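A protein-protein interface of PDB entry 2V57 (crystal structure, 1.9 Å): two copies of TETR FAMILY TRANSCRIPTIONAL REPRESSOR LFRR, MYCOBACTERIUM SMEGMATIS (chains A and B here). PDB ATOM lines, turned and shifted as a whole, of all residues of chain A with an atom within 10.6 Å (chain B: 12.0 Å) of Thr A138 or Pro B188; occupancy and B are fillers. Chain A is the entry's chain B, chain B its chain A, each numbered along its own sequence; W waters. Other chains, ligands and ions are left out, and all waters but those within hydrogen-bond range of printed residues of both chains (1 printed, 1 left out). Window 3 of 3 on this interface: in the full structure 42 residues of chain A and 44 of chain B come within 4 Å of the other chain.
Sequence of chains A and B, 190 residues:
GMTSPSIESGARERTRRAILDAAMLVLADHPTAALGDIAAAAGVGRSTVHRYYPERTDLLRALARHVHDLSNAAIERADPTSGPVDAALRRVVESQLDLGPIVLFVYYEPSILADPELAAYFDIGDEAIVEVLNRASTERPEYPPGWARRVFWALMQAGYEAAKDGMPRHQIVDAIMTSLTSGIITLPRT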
ATOM      1  N   GLY A  83      14.497  -5.439 -32.288  1.00  0.00           N
ATOM      2  CA  GLY A  83      14.117  -4.196 -31.630  1.00  0.00           C
ATOM      3  C   GLY A  83      14.571  -4.033 -30.188  1.00  0.00           C
ATOM      4  O   GLY A  83      15.412  -4.789 -29.703  1.00  0.00           O
ATOM      5  N   PRO A  84      14.023  -3.026 -29.492  1.00  0.00           N
ATOM      6  CA  PRO A  84      14.370  -2.732 -28.091  1.00  0.00           C
ATOM      7  C   PRO A  84      14.343  -3.979 -27.204  1.00  0.00           C
ATOM      8  O   PRO A  84      13.393  -4.756 -27.262  1.00  0.00           O
ATOM      9  CB  PRO A  84      13.270  -1.758 -27.660  1.00  0.00           C
ATOM     10  CG  PRO A  84      12.874  -1.065 -28.922  1.00  0.00           C
ATOM     11  CD  PRO A  84      13.035  -2.078 -30.034  1.00  0.00           C
ATOM     12  N   VAL A  85      15.379  -4.165 -26.388  1.00  0.00           N
ATOM     13  CA  VAL A  85      15.521  -5.407 -25.634  1.00  0.00           C
ATOM     14  C   VAL A  85      14.426  -5.588 -24.579  1.00  0.00           C
ATOM     15  O   VAL A  85      14.057  -6.713 -24.243  1.00  0.00           O
ATOM     16  CB  VAL A  85      16.911  -5.513 -24.962  1.00  0.00           C
ATOM     17  CG1 VAL A  85      18.020  -5.606 -26.021  1.00  0.00           C
ATOM     18  CG2 VAL A  85      17.129  -4.340 -24.027  1.00  0.00           C
ATOM     19  N   ASP A  86      13.898  -4.486 -24.056  1.00  0.00           N
ATOM     20  CA  ASP A  86      12.826  -4.588 -23.067  1.00  0.00           C
ATOM     21  C   ASP A  86      11.517  -5.102 -23.678  1.00  0.00           C
ATOM     22  O   ASP A  86      10.878  -5.996 -23.131  1.00  0.00           O
ATOM     23  CB  ASP A  86      12.608  -3.262 -22.339  1.00  0.00           C
ATOM     24  CG  ASP A  86      12.286  -2.117 -23.284  1.00  0.00           C
ATOM     25  OD1 ASP A  86      12.478  -2.260 -24.516  1.00  0.00           O
ATOM     26  OD2 ASP A  86      11.842  -1.063 -22.785  1.00  0.00           O
ATOM     27  N   ALA A  87      11.134  -4.547 -24.821  1.00  0.00           N
ATOM     28  CA  ALA A  87       9.959  -5.031 -25.533  1.00  0.00           C
ATOM     29  C   ALA A  87      10.154  -6.465 -26.009  1.00  0.00           C
ATOM     30  O   ALA A  87       9.205  -7.255 -26.002  1.00  0.00           O
ATOM     31  CB  ALA A  87       9.623  -4.121 -26.703  1.00  0.00           C
ATOM     32  N   ALA A  88      11.375  -6.802 -26.433  1.00  0.00           N
ATOM     33  CA  ALA A  88      11.661  -8.171 -26.861  1.00  0.00           C
ATOM     34  C   ALA A  88      11.497  -9.147 -25.705  1.00  0.00           C
ATOM     35  O   ALA A  88      10.870 -10.195 -25.860  1.00  0.00           O
ATOM     36  CB  ALA A  88      13.058  -8.279 -27.476  1.00  0.00           C
ATOM     37  N   LEU A  89      12.039  -8.792 -24.538  1.00  0.00           N
ATOM     38  CA  LEU A  89      11.909  -9.634 -23.351  1.00  0.00           C
ATOM     39  C   LEU A  89      10.435  -9.795 -22.982  1.00  0.00           C
ATOM     40  O   LEU A  89       9.997 -10.881 -22.621  1.00  0.00           O
ATOM     41  CB  LEU A  89      12.704  -9.056 -22.170  1.00  0.00           C
ATOM     42  CG  LEU A  89      12.654  -9.843 -20.856  1.00  0.00           C
ATOM     43  CD1 LEU A  89      13.067 -11.303 -21.061  1.00  0.00           C
ATOM     44  CD2 LEU A  89      13.497  -9.167 -19.751  1.00  0.00           C
ATOM     45  N   GLU A 131      20.338 -16.415 -23.014  1.00  0.00           N
ATOM     46  CA  GLU A 131      20.941 -15.479 -23.965  1.00  0.00           C
ATOM     47  C   GLU A 131      20.108 -14.224 -24.058  1.00  0.00           C
ATOM     48  O   GLU A 131      20.650 -13.116 -24.127  1.00  0.00           O
ATOM     49  CB  GLU A 131      21.085 -16.108 -25.365  1.00  0.00           C
ATOM     50  CG  GLU A 131      21.969 -17.319 -25.378  1.00  0.00           C
ATOM     51  CD  GLU A 131      23.408 -16.977 -25.053  1.00  0.00           C
ATOM     52  OE1 GLU A 131      23.875 -15.890 -25.461  1.00  0.00           O
ATOM     53  OE2 GLU A 131      24.074 -17.790 -24.374  1.00  0.00           O
ATOM     54  N   VAL A 132      18.790 -14.400 -24.076  1.00  0.00           N
ATOM     55  CA  VAL A 132      17.870 -13.275 -24.169  1.00  0.00           C
ATOM     56  C   VAL A 132      17.957 -12.390 -22.917  1.00  0.00           C
ATOM     57  O   VAL A 132      17.934 -11.165 -23.019  1.00  0.00           O
ATOM     58  CB  VAL A 132      16.405 -13.738 -24.366  1.00  0.00           C
ATOM     59  CG1 VAL A 132      15.444 -12.552 -24.215  1.00  0.00           C
ATOM     60  CG2 VAL A 132      16.231 -14.413 -25.730  1.00  0.00           C
ATOM     61  N   LEU A 133      18.070 -13.017 -21.748  1.00  0.00           N
ATOM     62  CA  LEU A 133      18.174 -12.275 -20.486  1.00  0.00           C
ATOM     63  C   LEU A 133      19.507 -11.540 -20.347  1.00  0.00           C
ATOM     64  O   LEU A 133      19.560 -10.365 -19.962  1.00  0.00           O
ATOM     65  CB  LEU A 133      17.978 -13.214 -19.300  1.00  0.00           C
ATOM     66  CG  LEU A 133      16.529 -13.640 -19.088  1.00  0.00           C
ATOM     67  CD1 LEU A 133      16.450 -14.914 -18.255  1.00  0.00           C
ATOM     68  CD2 LEU A 133      15.711 -12.500 -18.468  1.00  0.00           C
ATOM     69  N   ASN A 134      20.585 -12.243 -20.662  1.00  0.00           N
ATOM     70  CA  ASN A 134      21.918 -11.680 -20.551  1.00  0.00           C
ATOM     71  C   ASN A 134      22.127 -10.557 -21.542  1.00  0.00           C
ATOM     72  O   ASN A 134      22.833  -9.589 -21.265  1.00  0.00           O
ATOM     73  CB  ASN A 134      22.975 -12.755 -20.763  1.00  0.00           C
ATOM     74  CG  ASN A 134      23.050 -13.729 -19.608  1.00  0.00           C
ATOM     75  OD1 ASN A 134      22.046 -14.026 -18.957  1.00  0.00           O
ATOM     76  ND2 ASN A 134      24.246 -14.234 -19.342  1.00  0.00           N
ATOM     77  N   ARG A 135      21.501 -10.676 -22.700  1.00  0.00           N
ATOM     78  CA  ARG A 135      21.708  -9.651 -23.698  1.00  0.00           C
ATOM     79  C   ARG A 135      20.708  -8.496 -23.521  1.00  0.00           C
ATOM     80  O   ARG A 135      20.702  -7.537 -24.287  1.00  0.00           O
ATOM     81  CB  ARG A 135      21.764 -10.281 -25.097  1.00  0.00           C
ATOM     82  CG  ARG A 135      22.939 -11.276 -25.200  1.00  0.00           C
ATOM     83  CD  ARG A 135      22.874 -12.213 -26.410  1.00  0.00           C
ATOM     84  NE  ARG A 135      23.910 -13.239 -26.319  1.00  0.00           N
ATOM     85  CZ  ARG A 135      25.115 -13.153 -26.877  1.00  0.00           C
ATOM     86  NH1 ARG A 135      25.455 -12.093 -27.611  1.00  0.00           N
ATOM     87  NH2 ARG A 135      25.981 -14.145 -26.720  1.00  0.00           N
ATOM     88  N   ALA A 136      19.913  -8.568 -22.455  1.00  0.00           N
ATOM     89  CA  ALA A 136      19.062  -7.445 -22.077  1.00  0.00           C
ATOM     90  C   ALA A 136      19.571  -6.800 -20.791  1.00  0.00           C
ATOM     91  O   ALA A 136      18.924  -5.906 -20.237  1.00  0.00           O
ATOM     92  CB  ALA A 136      17.629  -7.892 -21.903  1.00  0.00           C
ATOM     93  N   SER A 137      20.721  -7.260 -20.306  1.00  0.00           N
ATOM     94  CA  SER A 137      21.209  -6.808 -19.004  1.00  0.00           C
ATOM     95  C   SER A 137      22.539  -6.090 -19.101  1.00  0.00           C
ATOM     96  O   SER A 137      23.434  -6.518 -19.832  1.00  0.00           O
ATOM     97  CB  SER A 137      21.338  -7.974 -18.028  1.00  0.00           C
ATOM     98  OG  SER A 137      21.637  -7.495 -16.727  1.00  0.00           O
ATOM     99  N   THR A 138      22.662  -5.006 -18.339  1.00  0.00           N
ATOM    100  CA  THR A 138      23.858  -4.173 -18.357  1.00  0.00           C
ATOM    101  C   THR A 138      24.908  -4.672 -17.360  1.00  0.00           C
ATOM    102  O   THR A 138      26.051  -4.215 -17.373  1.00  0.00           O
ATOM    103  CB  THR A 138      23.530  -2.694 -18.042  1.00  0.00           C
ATOM    104  OG1 THR A 138      23.042  -2.587 -16.703  1.00  0.00           O
ATOM    105  CG2 THR A 138      22.476  -2.136 -19.010  1.00  0.00           C
ATOM    106  N   GLU A 139      24.521  -5.609 -16.500  1.00  0.00           N
ATOM    107  CA  GLU A 139      25.448  -6.171 -15.518  1.00  0.00           C
ATOM    108  C   GLU A 139      25.576  -7.683 -15.677  1.00  0.00           C
ATOM    109  O   GLU A 139      24.979  -8.263 -16.579  1.00  0.00           O
ATOM    110  CB  GLU A 139      24.982  -5.849 -14.098  1.00  0.00           C
ATOM    111  CG  GLU A 139      24.997  -4.377 -13.748  1.00  0.00           C
ATOM    112  CD  GLU A 139      24.869  -4.144 -12.254  1.00  0.00           C
ATOM    113  OE1 GLU A 139      24.207  -4.964 -11.579  1.00  0.00           O
ATOM    114  OE2 GLU A 139      25.435  -3.144 -11.756  1.00  0.00           O
ATOM    115  N   ARG A 140      26.352  -8.313 -14.794  1.00  0.00           N
ATOM    116  CA  ARG A 140      26.417  -9.771 -14.727  1.00  0.00           C
ATOM    117  C   ARG A 140      25.878 -10.293 -13.390  1.00  0.00           C
ATOM    118  O   ARG A 140      26.144 -11.431 -12.988  1.00  0.00           O
ATOM    119  CB  ARG A 140      27.849 -10.262 -14.956  1.00  0.00           C
ATOM    120  N   MET A 177       7.868  -9.002 -15.505  1.00  0.00           N
ATOM    121  CA  MET A 177       8.897  -8.091 -16.027  1.00  0.00           C
ATOM    122  C   MET A 177       9.558  -7.285 -14.901  1.00  0.00           C
ATOM    123  O   MET A 177      10.785  -7.163 -14.846  1.00  0.00           O
ATOM    124  CB  MET A 177       8.329  -7.150 -17.098  1.00  0.00           C
ATOM    125  CG  MET A 177       8.045  -7.808 -18.425  1.00  0.00           C
ATOM    126  SD  MET A 177       9.545  -8.402 -19.244  1.00  0.00           S
ATOM    127  CE  MET A 177      10.389  -6.861 -19.645  1.00  0.00           C
ATOM    128  N   LEU A 180      11.821  -9.534 -12.716  1.00  0.00           N
ATOM    129  CA  LEU A 180      13.077  -9.862 -13.379  1.00  0.00           C
ATOM    130  C   LEU A 180      14.086  -8.707 -13.278  1.00  0.00           C
ATOM    131  O   LEU A 180      15.280  -8.918 -13.037  1.00  0.00           O
ATOM    132  CB  LEU A 180      12.838 -10.212 -14.865  1.00  0.00           C
ATOM    133  CG  LEU A 180      12.180 -11.577 -15.133  1.00  0.00           C
ATOM    134  CD1 LEU A 180      11.594 -11.662 -16.554  1.00  0.00           C
ATOM    135  CD2 LEU A 180      13.162 -12.736 -14.865  1.00  0.00           C
ATOM    136  N   THR A 181      13.591  -7.486 -13.445  1.00  0.00           N
ATOM    137  CA  THR A 181      14.470  -6.335 -13.627  1.00  0.00           C
ATOM    138  C   THR A 181      14.676  -5.485 -12.371  1.00  0.00           C
ATOM    139  O   THR A 181      15.471  -4.540 -12.396  1.00  0.00           O
ATOM    140  CB  THR A 181      13.931  -5.406 -14.747  1.00  0.00           C
ATOM    141  OG1 THR A 181      12.677  -4.850 -14.347  1.00  0.00           O
ATOM    142  CG2 THR A 181      13.727  -6.186 -16.050  1.00  0.00           C
ATOM    143  N   SER B 182      17.058  -6.827  -6.158  1.00  0.00           N
ATOM    144  CA  SER B 182      17.517  -6.266  -7.433  1.00  0.00           C
ATOM    145  C   SER B 182      16.981  -6.962  -8.686  1.00  0.00           C
ATOM    146  O   SER B 182      17.138  -6.442  -9.786  1.00  0.00           O
ATOM    147  CB  SER B 182      19.052  -6.308  -7.488  1.00  0.00           C
ATOM    148  OG  SER B 182      19.603  -5.807  -6.288  1.00  0.00           O
ATOM    149  N   GLY B 183      16.369  -8.135  -8.532  1.00  0.00           N
ATOM    150  CA  GLY B 183      15.971  -8.916  -9.691  1.00  0.00           C
ATOM    151  C   GLY B 183      17.200  -9.601 -10.279  1.00  0.00           C
ATOM    152  O   GLY B 183      18.245  -9.668  -9.628  1.00  0.00           O
ATOM    153  N   ILE B 184      17.098 -10.125 -11.494  1.00  0.00           N
ATOM    154  CA  ILE B 184      18.241 -10.833 -12.055  1.00  0.00           C
ATOM    155  C   ILE B 184      18.890 -10.142 -13.234  1.00  0.00           C
ATOM    156  O   ILE B 184      19.955 -10.566 -13.655  1.00  0.00           O
ATOM    157  CB  ILE B 184      17.925 -12.294 -12.440  1.00  0.00           C
ATOM    158  CG1 ILE B 184      16.685 -12.376 -13.321  1.00  0.00           C
ATOM    159  CG2 ILE B 184      17.740 -13.142 -11.196  1.00  0.00           C
ATOM    160  CD1 ILE B 184      16.577 -13.709 -14.092  1.00  0.00           C
ATOM    161  N   ILE B 185      18.254  -9.102 -13.768  1.00  0.00           N
ATOM    162  CA  ILE B 185      18.851  -8.316 -14.851  1.00  0.00           C
ATOM    163  C   ILE B 185      18.657  -6.830 -14.586  1.00  0.00           C
ATOM    164  O   ILE B 185      17.863  -6.447 -13.735  1.00  0.00           O
ATOM    165  CB  ILE B 185      18.261  -8.664 -16.230  1.00  0.00           C
ATOM    166  CG1 ILE B 185      16.768  -8.356 -16.272  1.00  0.00           C
ATOM    167  CG2 ILE B 185      18.536 -10.133 -16.573  1.00  0.00           C
ATOM    168  CD1 ILE B 185      16.212  -8.189 -17.678  1.00  0.00           C
ATOM    169  N   THR B 186      19.404  -5.999 -15.299  1.00  0.00           N
ATOM    170  CA  THR B 186      19.262  -4.559 -15.163  1.00  0.00           C
ATOM    171  C   THR B 186      19.118  -3.992 -16.560  1.00  0.00           C
ATOM    172  O   THR B 186      20.032  -4.094 -17.371  1.00  0.00           O
ATOM    173  CB  THR B 186      20.479  -3.926 -14.461  1.00  0.00           C
ATOM    174  OG1 THR B 186      20.645  -4.534 -13.176  1.00  0.00           O
ATOM    175  CG2 THR B 186      20.286  -2.420 -14.282  1.00  0.00           C
ATOM    176  N   LEU B 187      17.956  -3.423 -16.847  1.00  0.00           N
ATOM    177  CA  LEU B 187      17.694  -2.854 -18.163  1.00  0.00           C
ATOM    178  C   LEU B 187      18.425  -1.531 -18.355  1.00  0.00           C
ATOM    179  O   LEU B 187      18.649  -0.792 -17.393  1.00  0.00           O
ATOM    180  CB  LEU B 187      16.196  -2.654 -18.371  1.00  0.00           C
ATOM    181  CG  LEU B 187      15.367  -3.935 -18.398  1.00  0.00           C
ATOM    182  CD1 LEU B 187      13.897  -3.608 -18.582  1.00  0.00           C
ATOM    183  CD2 LEU B 187      15.862  -4.854 -19.495  1.00  0.00           C
ATOM    184  N   PRO B 188      18.815  -1.237 -19.605  1.00  0.00           N
ATOM    185  CA  PRO B 188      19.386   0.072 -19.949  1.00  0.00           C
ATOM    186  C   PRO B 188      18.387   1.192 -19.695  1.00  0.00           C
ATOM    187  O   PRO B 188      18.656   2.055 -18.862  1.00  0.00           O
ATOM    188  CB  PRO B 188      19.648  -0.038 -21.452  1.00  0.00           C
ATOM    189  CG  PRO B 188      19.657  -1.483 -21.752  1.00  0.00           C
ATOM    190  CD  PRO B 188      18.772  -2.155 -20.753  1.00  0.00           C
HETATM  191  O   HOH W   1      16.169  -2.760 -14.636  1.00  0.00           O
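The backbone NH (N) of Ile B184 sits at hydrogen-bond distance from the backbone carbonyl oxygen (O) of Leu A180, 2.7 Å away. The backbone NH (N) of Ile B185 lies within hydrogen-bond range of the backbone carbonyl oxygen (O) of Leu A180, 3.1 Å away. N of Thr B186 is in hydrogen-bond range of OG of Ser A137, 3.0 Å away. N of Thr A138 is in hydrogen-bond range of O of Thr B186 (2.9 Å). The backbone carbonyl oxygen of Thr A181 lies close to the backbone carbonyl oxygen of Ile B185 (3.3 Å).
The side-chain hydroxyl (OG) of Ser A137 lies within hydrogen-bond range of the backbone carbonyl oxygen (O) of Glu A139 (3.4 Å). The side-chain hydroxyl (OG1) of Thr A181 is in hydrogen-bond range of the backbone carbonyl oxygen (O) of Met A177 (3.0 Å).
CD1 of Leu B187 touches CB of Asp A86, at 3.99 Å. CD1 of Ile B185 touches CD2 of Leu A89 (3.6 Å). CG2 of Ile B185 touches O of Leu A133, at 3.5 Å. Ala A136 touches Thr B186. CD of Pro B188 touches O of Ala A136 (3.8 Å). Ser A137 touches Ile B185. N of Pro B188 touches CG2 of Thr A138, at 3.8 Å. OE1 of Glu A139 touches OG1 of Thr B186, 3.9 Å away. O of Leu A180 touches CA of Gly B183, at 3.4 Å. Thr A181 touches Ser B182.
No residue of chain B comes within 4 Å of Val A85. Of the printed residues of chain B, Leu A89 touches Ile B185. Glu A131 touches none of the printed residues of chain B. Printed residues of chain B within 4 Å of Ala A136: Thr B186 (3.6 Å), Leu B187 (3.3 Å) and Pro B188 (3.8 Å). Ser A137 touches just these residues of chain B: Ile B185 and Thr B186. Of chain B, only Thr B186 (2.9 Å) and Pro B188 (3.8 Å) come within 4 Å of Thr A138. Of the printed residues of chain B, Glu A139 touches Thr B186. Met A177 touches none of the printed residues of chain B. Printed residues of chain B within 4 Å of Leu A180: Gly B183 (3.4 Å), Ile B184 (2.7 Å) and Ile B185 (3.1 Å). Printed residues of chain B within 4 Å of Thr A181: Ser B182, Ile B185 and Leu B187. Printed residues of chain A within 4 Å of Ser B182: Thr A181. Of the printed residues of chain A, Ile B185 touches Leu A89 (3.6 Å), Leu A133 (3.5 Å), Ser A137 (3.5 Å), Leu A180 (3.1 Å) and Thr A181 (3.3 Å). The nearest residue of chain B that does not touch Thr A138 is Leu B187 (4.1 Å). The nearest printed residue of chain B that does not touch Thr A181 is Gly B183 (4.5 Å).
Hydrophobic or aromatic side chains of chain A that line the printed part of chain B: Leu A89 and Leu A180. Along chain A the printed residues that touch a printed residue of chain B span positions 86 to 181. Hydrophobic or aromatic side chains of chain B within 4 Å of the printed part of chain A: Ile B184, Ile B185, Leu B187 and Pro B188. Among the printed residues, no Asp or Glu carboxylate lies within 4 Å of a Lys or Arg side-chain nitrogen of the other chain.
No position is printed for both chains.
Water W1 lies within hydrogen-bond range of N of Leu B187 (2.9 Å) and O of Thr A181 (2.9 Å).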
